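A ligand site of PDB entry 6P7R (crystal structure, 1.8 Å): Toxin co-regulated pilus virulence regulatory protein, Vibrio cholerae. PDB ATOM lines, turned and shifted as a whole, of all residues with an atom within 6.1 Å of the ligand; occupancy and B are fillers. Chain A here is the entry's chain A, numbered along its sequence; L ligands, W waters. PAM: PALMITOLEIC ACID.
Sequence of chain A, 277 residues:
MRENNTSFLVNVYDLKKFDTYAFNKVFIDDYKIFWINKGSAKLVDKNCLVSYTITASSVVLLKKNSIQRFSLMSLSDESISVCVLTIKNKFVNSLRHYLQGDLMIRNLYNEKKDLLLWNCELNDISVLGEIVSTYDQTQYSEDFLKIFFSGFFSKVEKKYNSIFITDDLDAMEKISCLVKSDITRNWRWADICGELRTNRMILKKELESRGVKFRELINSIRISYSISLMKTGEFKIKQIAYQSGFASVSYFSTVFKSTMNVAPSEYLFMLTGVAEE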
ATOM      1  N   ASN A  11      19.039  12.607 -21.037  1.00  0.00           N
ATOM      2  CA  ASN A  11      19.346  11.712 -19.922  1.00  0.00           C
ATOM      3  C   ASN A  11      20.039  12.520 -18.849  1.00  0.00           C
ATOM      4  O   ASN A  11      20.937  13.311 -19.158  1.00  0.00           O
ATOM      5  CB  ASN A  11      20.247  10.548 -20.368  1.00  0.00           C
ATOM      6  CG  ASN A  11      19.583   9.679 -21.415  1.00  0.00           C
ATOM      7  OD1 ASN A  11      19.861   9.817 -22.603  1.00  0.00           O
ATOM      8  ND2 ASN A  11      18.674   8.809 -20.982  1.00  0.00           N
ATOM      9  N   TYR A  13      22.015  12.239 -15.057  1.00  0.00           N
ATOM     10  CA  TYR A  13      22.730  11.288 -14.213  1.00  0.00           C
ATOM     11  C   TYR A  13      23.183  11.988 -12.948  1.00  0.00           C
ATOM     12  O   TYR A  13      23.615  13.142 -12.994  1.00  0.00           O
ATOM     13  CB  TYR A  13      23.961  10.734 -14.951  1.00  0.00           C
ATOM     14  CG  TYR A  13      23.624  10.013 -16.235  1.00  0.00           C
ATOM     15  CD1 TYR A  13      23.140   8.715 -16.214  1.00  0.00           C
ATOM     16  CD2 TYR A  13      23.791  10.632 -17.470  1.00  0.00           C
ATOM     17  CE1 TYR A  13      22.833   8.039 -17.377  1.00  0.00           C
ATOM     18  CE2 TYR A  13      23.471   9.970 -18.648  1.00  0.00           C
ATOM     19  CZ  TYR A  13      23.010   8.667 -18.592  1.00  0.00           C
ATOM     20  OH  TYR A  13      22.702   7.980 -19.763  1.00  0.00           O
ATOM     21  N   LEU A  15      25.663  12.779 -10.029  1.00  0.00           N
ATOM     22  CA  LEU A  15      27.099  12.795  -9.738  1.00  0.00           C
ATOM     23  C   LEU A  15      27.231  13.100  -8.245  1.00  0.00           C
ATOM     24  O   LEU A  15      27.084  14.251  -7.824  1.00  0.00           O
ATOM     25  CB  LEU A  15      27.814  13.838 -10.591  1.00  0.00           C
ATOM     26  CG  LEU A  15      29.292  14.129 -10.277  1.00  0.00           C
ATOM     27  CD1 LEU A  15      30.147  12.870 -10.366  1.00  0.00           C
ATOM     28  CD2 LEU A  15      29.833  15.215 -11.198  1.00  0.00           C
ATOM     29  N   TYR A  21      33.473  10.027 -12.476  1.00  0.00           N
ATOM     30  CA  TYR A  21      33.171   9.180 -13.620  1.00  0.00           C
ATOM     31  C   TYR A  21      34.390   9.185 -14.545  1.00  0.00           C
ATOM     32  O   TYR A  21      34.938  10.249 -14.855  1.00  0.00           O
ATOM     33  CB  TYR A  21      31.953   9.696 -14.395  1.00  0.00           C
ATOM     34  CG  TYR A  21      30.584   9.545 -13.738  1.00  0.00           C
ATOM     35  CD1 TYR A  21      30.081   8.296 -13.420  1.00  0.00           C
ATOM     36  CD2 TYR A  21      29.796  10.658 -13.490  1.00  0.00           C
ATOM     37  CE1 TYR A  21      28.812   8.165 -12.842  1.00  0.00           C
ATOM     38  CE2 TYR A  21      28.543  10.543 -12.912  1.00  0.00           C
ATOM     39  CZ  TYR A  21      28.050   9.291 -12.592  1.00  0.00           C
ATOM     40  OH  TYR A  21      26.804   9.161 -12.021  1.00  0.00           O
ATOM     41  N   PHE A  23      35.885   7.565 -18.319  1.00  0.00           N
ATOM     42  CA  PHE A  23      35.500   6.898 -19.548  1.00  0.00           C
ATOM     43  C   PHE A  23      36.734   6.538 -20.349  1.00  0.00           C
ATOM     44  O   PHE A  23      37.609   7.391 -20.558  1.00  0.00           O
ATOM     45  CB  PHE A  23      34.549   7.775 -20.358  1.00  0.00           C
ATOM     46  CG  PHE A  23      33.364   8.244 -19.567  1.00  0.00           C
ATOM     47  CD1 PHE A  23      32.280   7.400 -19.374  1.00  0.00           C
ATOM     48  CD2 PHE A  23      33.344   9.496 -18.987  1.00  0.00           C
ATOM     49  CE1 PHE A  23      31.188   7.801 -18.618  1.00  0.00           C
ATOM     50  CE2 PHE A  23      32.249   9.918 -18.235  1.00  0.00           C
ATOM     51  CZ  PHE A  23      31.173   9.060 -18.048  1.00  0.00           C
ATOM     52  N   VAL A  26      35.312   5.417 -24.976  1.00  0.00           N
ATOM     53  CA  VAL A  26      33.878   5.406 -25.217  1.00  0.00           C
ATOM     54  C   VAL A  26      33.597   5.963 -26.610  1.00  0.00           C
ATOM     55  O   VAL A  26      34.097   7.025 -27.000  1.00  0.00           O
ATOM     56  CB  VAL A  26      33.120   6.205 -24.121  1.00  0.00           C
ATOM     57  CG1 VAL A  26      33.663   7.582 -24.000  1.00  0.00           C
ATOM     58  CG2 VAL A  26      31.584   6.233 -24.426  1.00  0.00           C
ATOM     59  N   ILE A  28      31.251   7.682 -29.234  1.00  0.00           N
ATOM     60  CA  ILE A  28      30.137   8.636 -29.252  1.00  0.00           C
ATOM     61  C   ILE A  28      29.312   8.357 -30.496  1.00  0.00           C
ATOM     62  O   ILE A  28      29.694   8.734 -31.604  1.00  0.00           O
ATOM     63  CB  ILE A  28      30.648  10.091 -29.212  1.00  0.00           C
ATOM     64  CG1 ILE A  28      31.585  10.314 -28.022  1.00  0.00           C
ATOM     65  CG2 ILE A  28      29.493  11.080 -29.139  1.00  0.00           C
ATOM     66  CD1 ILE A  28      30.953  10.088 -26.632  1.00  0.00           C
ATOM     67  N   LYS A  32      26.543  14.814 -28.942  1.00  0.00           N
ATOM     68  CA  LYS A  32      26.063  14.968 -27.579  1.00  0.00           C
ATOM     69  C   LYS A  32      26.593  16.261 -26.995  1.00  0.00           C
ATOM     70  O   LYS A  32      27.720  16.655 -27.271  1.00  0.00           O
ATOM     71  CB  LYS A  32      26.511  13.810 -26.664  1.00  0.00           C
ATOM     72  CG  LYS A  32      25.837  12.503 -26.962  1.00  0.00           C
ATOM     73  CD  LYS A  32      26.370  11.406 -26.094  1.00  0.00           C
ATOM     74  CE  LYS A  32      25.894  10.058 -26.618  1.00  0.00           C
ATOM     75  NZ  LYS A  32      24.537   9.704 -26.121  1.00  0.00           N
ATOM     76  N   PHE A  34      26.683  18.160 -22.968  1.00  0.00           N
ATOM     77  CA  PHE A  34      26.305  17.918 -21.584  1.00  0.00           C
ATOM     78  C   PHE A  34      26.731  19.086 -20.719  1.00  0.00           C
ATOM     79  O   PHE A  34      27.578  19.898 -21.102  1.00  0.00           O
ATOM     80  CB  PHE A  34      26.845  16.562 -21.032  1.00  0.00           C
ATOM     81  CG  PHE A  34      28.341  16.478 -20.775  1.00  0.00           C
ATOM     82  CD1 PHE A  34      28.890  16.935 -19.576  1.00  0.00           C
ATOM     83  CD2 PHE A  34      29.188  15.869 -21.702  1.00  0.00           C
ATOM     84  CE1 PHE A  34      30.249  16.812 -19.337  1.00  0.00           C
ATOM     85  CE2 PHE A  34      30.543  15.737 -21.462  1.00  0.00           C
ATOM     86  CZ  PHE A  34      31.083  16.228 -20.270  1.00  0.00           C
ATOM     87  N   LEU A  62      30.486  16.830 -27.593  1.00  0.00           N
ATOM     88  CA  LEU A  62      31.182  15.600 -27.939  1.00  0.00           C
ATOM     89  C   LEU A  62      30.836  15.270 -29.382  1.00  0.00           C
ATOM     90  O   LEU A  62      29.660  15.157 -29.726  1.00  0.00           O
ATOM     91  CB  LEU A  62      30.780  14.443 -27.024  1.00  0.00           C
ATOM     92  CG  LEU A  62      31.048  14.731 -25.536  1.00  0.00           C
ATOM     93  CD1 LEU A  62      30.548  13.604 -24.663  1.00  0.00           C
ATOM     94  CD2 LEU A  62      32.543  14.948 -25.361  1.00  0.00           C
ATOM     95  N   PHE A  70      38.160  10.423 -20.979  1.00  0.00           N
ATOM     96  CA  PHE A  70      38.154  11.557 -20.058  1.00  0.00           C
ATOM     97  C   PHE A  70      37.543  11.157 -18.728  1.00  0.00           C
ATOM     98  O   PHE A  70      36.918  10.103 -18.587  1.00  0.00           O
ATOM     99  CB  PHE A  70      37.436  12.776 -20.690  1.00  0.00           C
ATOM    100  CG  PHE A  70      35.929  12.634 -20.797  1.00  0.00           C
ATOM    101  CD1 PHE A  70      35.090  13.038 -19.773  1.00  0.00           C
ATOM    102  CD2 PHE A  70      35.356  12.157 -21.966  1.00  0.00           C
ATOM    103  CE1 PHE A  70      33.709  12.947 -19.889  1.00  0.00           C
ATOM    104  CE2 PHE A  70      33.964  12.058 -22.092  1.00  0.00           C
ATOM    105  CZ  PHE A  70      33.140  12.459 -21.044  1.00  0.00           C
ATOM    106  N   LEU A  72      35.417  12.945 -15.160  1.00  0.00           N
ATOM    107  CA  LEU A  72      34.656  14.068 -14.632  1.00  0.00           C
ATOM    108  C   LEU A  72      34.529  13.846 -13.137  1.00  0.00           C
ATOM    109  O   LEU A  72      34.006  12.808 -12.704  1.00  0.00           O
ATOM    110  CB  LEU A  72      33.275  14.164 -15.293  1.00  0.00           C
ATOM    111  CG  LEU A  72      32.453  15.408 -14.939  1.00  0.00           C
ATOM    112  CD1 LEU A  72      33.158  16.669 -15.471  1.00  0.00           C
ATOM    113  CD2 LEU A  72      30.990  15.281 -15.463  1.00  0.00           C
ATOM    114  N   VAL A  82      24.142  15.691 -13.924  1.00  0.00           N
ATOM    115  CA  VAL A  82      24.753  15.869 -15.238  1.00  0.00           C
ATOM    116  C   VAL A  82      23.689  15.621 -16.281  1.00  0.00           C
ATOM    117  O   VAL A  82      23.117  14.527 -16.340  1.00  0.00           O
ATOM    118  CB  VAL A  82      25.958  14.931 -15.464  1.00  0.00           C
ATOM    119  CG1 VAL A  82      26.588  15.281 -16.803  1.00  0.00           C
ATOM    120  CG2 VAL A  82      26.968  15.068 -14.340  1.00  0.00           C
ATOM    121  N   VAL A  84      22.661  15.210 -20.137  1.00  0.00           N
ATOM    122  CA  VAL A  84      23.273  14.808 -21.395  1.00  0.00           C
ATOM    123  C   VAL A  84      22.198  14.870 -22.461  1.00  0.00           C
ATOM    124  O   VAL A  84      21.209  14.127 -22.402  1.00  0.00           O
ATOM    125  CB  VAL A  84      23.867  13.392 -21.317  1.00  0.00           C
ATOM    126  CG1 VAL A  84      24.504  13.047 -22.653  1.00  0.00           C
ATOM    127  CG2 VAL A  84      24.853  13.286 -20.157  1.00  0.00           C
ATOM    128  N   THR A  86      21.345  14.251 -26.294  1.00  0.00           N
ATOM    129  CA  THR A  86      21.796  13.571 -27.483  1.00  0.00           C
ATOM    130  C   THR A  86      20.974  14.110 -28.646  1.00  0.00           C
ATOM    131  O   THR A  86      19.749  14.177 -28.556  1.00  0.00           O
ATOM    132  CB  THR A  86      21.607  12.051 -27.375  1.00  0.00           C
ATOM    133  OG1 THR A  86      22.396  11.559 -26.287  1.00  0.00           O
ATOM    134  CG2 THR A  86      22.065  11.358 -28.663  1.00  0.00           C
ATOM    135  N   ILE A 227      24.261   0.487 -24.648  1.00  0.00           N
ATOM    136  CA  ILE A 227      23.665   1.613 -23.939  1.00  0.00           C
ATOM    137  C   ILE A 227      22.433   2.119 -24.663  1.00  0.00           C
ATOM    138  O   ILE A 227      21.429   2.476 -24.028  1.00  0.00           O
ATOM    139  CB  ILE A 227      24.715   2.713 -23.749  1.00  0.00           C
ATOM    140  CG1 ILE A 227      25.709   2.288 -22.657  1.00  0.00           C
ATOM    141  CG2 ILE A 227      24.031   4.065 -23.421  1.00  0.00           C
ATOM    142  CD1 ILE A 227      26.934   3.154 -22.584  1.00  0.00           C
ATOM    143  N   LYS A 231      18.477   2.220 -23.180  1.00  0.00           N
ATOM    144  CA  LYS A 231      17.595   3.385 -23.255  1.00  0.00           C
ATOM    145  C   LYS A 231      16.269   3.096 -23.955  1.00  0.00           C
ATOM    146  O   LYS A 231      15.295   3.825 -23.727  1.00  0.00           O
ATOM    147  CB  LYS A 231      18.322   4.524 -23.968  1.00  0.00           C
ATOM    148  CG  LYS A 231      19.398   5.143 -23.108  1.00  0.00           C
ATOM    149  CD  LYS A 231      20.155   6.212 -23.867  1.00  0.00           C
ATOM    150  CE  LYS A 231      21.237   6.831 -22.985  1.00  0.00           C
ATOM    151  NZ  LYS A 231      21.777   8.050 -23.661  1.00  0.00           N
ATOM    152  N   MET A 260      33.204   2.100 -19.161  1.00  0.00           N
ATOM    153  CA  MET A 260      32.351   3.043 -18.434  1.00  0.00           C
ATOM    154  C   MET A 260      32.710   3.169 -16.965  1.00  0.00           C
ATOM    155  O   MET A 260      32.155   4.044 -16.279  1.00  0.00           O
ATOM    156  CB  MET A 260      30.881   2.609 -18.559  1.00  0.00           C
ATOM    157  CG  MET A 260      30.461   2.316 -19.999  1.00  0.00           C
ATOM    158  SD  MET A 260      30.499   3.828 -20.983  1.00  0.00           S
ATOM    159  CE  MET A 260      29.246   4.760 -20.168  1.00  0.00           C
ATOM    160  N   TYR A 267      24.999   0.865 -14.248  1.00  0.00           N
ATOM    161  CA  TYR A 267      24.562   1.853 -15.226  1.00  0.00           C
ATOM    162  C   TYR A 267      23.051   1.810 -15.412  1.00  0.00           C
ATOM    163  O   TYR A 267      22.396   2.861 -15.512  1.00  0.00           O
ATOM    164  CB  TYR A 267      25.268   1.673 -16.577  1.00  0.00           C
ATOM    165  CG  TYR A 267      24.638   2.608 -17.589  1.00  0.00           C
ATOM    166  CD1 TYR A 267      24.884   3.987 -17.529  1.00  0.00           C
ATOM    167  CD2 TYR A 267      23.716   2.152 -18.512  1.00  0.00           C
ATOM    168  CE1 TYR A 267      24.260   4.858 -18.416  1.00  0.00           C
ATOM    169  CE2 TYR A 267      23.093   3.003 -19.385  1.00  0.00           C
ATOM    170  CZ  TYR A 267      23.352   4.356 -19.329  1.00  0.00           C
ATOM    171  OH  TYR A 267      22.729   5.207 -20.203  1.00  0.00           O
ATOM    172  N   MET A 270      21.623   3.807 -12.686  1.00  0.00           N
ATOM    173  CA  MET A 270      21.799   5.240 -12.956  1.00  0.00           C
ATOM    174  C   MET A 270      20.804   5.723 -14.006  1.00  0.00           C
ATOM    175  O   MET A 270      20.287   6.844 -13.899  1.00  0.00           O
ATOM    176  CB  MET A 270      23.231   5.518 -13.418  1.00  0.00           C
ATOM    177  CG  MET A 270      24.286   5.248 -12.373  1.00  0.00           C
ATOM    178  SD  MET A 270      25.956   5.202 -13.079  1.00  0.00           S
ATOM    179  CE  MET A 270      25.891   6.597 -14.206  1.00  0.00           C
HETATM  180  C1  PAM L   1      24.769   8.123 -22.592  1.00  0.00           C
HETATM  181  O1  PAM L   1      25.021   8.148 -23.828  1.00  0.00           O
HETATM  182  O2  PAM L   1      23.821   8.806 -22.116  1.00  0.00           O
HETATM  183  C2  PAM L   1      25.635   7.243 -21.694  1.00  0.00           C
HETATM  184  C3  PAM L   1      25.944   7.986 -20.398  1.00  0.00           C
HETATM  185  C4  PAM L   1      27.300   7.509 -19.895  1.00  0.00           C
HETATM  186  C5  PAM L   1      27.401   7.667 -18.383  1.00  0.00           C
HETATM  187  C6  PAM L   1      26.804   9.013 -18.018  1.00  0.00           C
HETATM  188  C7  PAM L   1      27.003   9.282 -16.539  1.00  0.00           C
HETATM  189  C8  PAM L   1      28.294  10.055 -16.418  1.00  0.00           C
HETATM  190  C9  PAM L   1      27.957  11.507 -16.100  1.00  0.00           C
HETATM  191  C10 PAM L   1      28.377  12.492 -16.870  1.00  0.00           C
HETATM  192  C11 PAM L   1      29.194  12.283 -18.136  1.00  0.00           C
HETATM  193  C12 PAM L   1      28.334  12.815 -19.285  1.00  0.00           C
HETATM  194  C13 PAM L   1      28.944  12.497 -20.650  1.00  0.00           C
HETATM  195  C14 PAM L   1      28.771  11.014 -20.947  1.00  0.00           C
HETATM  196  C15 PAM L   1      29.137  10.739 -22.412  1.00  0.00           C
HETATM  197  C16 PAM L   1      29.916   9.424 -22.483  1.00  0.00           C
HETATM  198  O   HOH W   1      26.645   6.107 -25.620  1.00  0.00           O
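The side-chain amino group (NZ) of Lys 231 lies within salt-bridge range of an oxygen (O2) of the ligand (2.7 Å).
OH of Tyr 13 is in hydrogen-bond range of O2 of the ligand (2.7 Å).
The side-chain amino group (NZ) of Lys 32 is in salt-bridge range of an oxygen (O1) of the ligand, at 2.8 Å.
The side-chain amino group (NZ) of Lys 231 sits at hydrogen-bond distance from the side-chain amide oxygen (OD1) of Asn 11 (2.8 Å).
The backbone carbonyl oxygen (O) of Tyr 13 is in hydrogen-bond range of the backbone NH (N) of Val 82.
OH of Tyr 267 lies within hydrogen-bond range of OH of Tyr 13 (2.8 Å).
The backbone carbonyl oxygen (O) of Lys 32 sits at hydrogen-bond distance from the backbone NH (N) of Leu 62 (2.8 Å).
NZ of Lys 32 is in hydrogen-bond range of OG1 of Thr 86 (2.8 Å).
N of Leu 72 sits at hydrogen-bond distance from O of Tyr 21, 2.8 Å away.
N of Phe 23 is in hydrogen-bond range of O of Phe 70, 2.8 Å away.
The backbone NH of Val 84 lies within hydrogen-bond range of the backbone carbonyl oxygen of Asn 11 (2.7 Å).
Tyr 21 touches the ligand (CD2 to C9, 3.3 Å).
Phe 23 touches the ligand.
CD2 of Phe 34 touches C13 of the ligand, 3.5 Å away.
Leu 62 touches the ligand (CD1 to C15, 3.9 Å).
Val 82 touches the ligand.
CG2 of Val 84 touches C12 of the ligand, 3.6 Å away.
CG2 of Ile 227 touches C2 of the ligand (3.96 Å).
CE of Met 260 touches C4 of the ligand (3.4 Å).
Tyr 267 touches the ligand (OH to C2, 3.8 Å).
Met 270 touches the ligand (CE to C7, 3.7 Å).
Within 4 Å of the ligand: Tyr 13, Tyr 21, Phe 23, Lys 32, Phe 34, Leu 62, Val 82, Val 84, Ile 227, Lys 231, Met 260, Tyr 267 and Met 270.
The nearest printed residue that does not touch the ligand is Leu 72 (4.1 Å).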
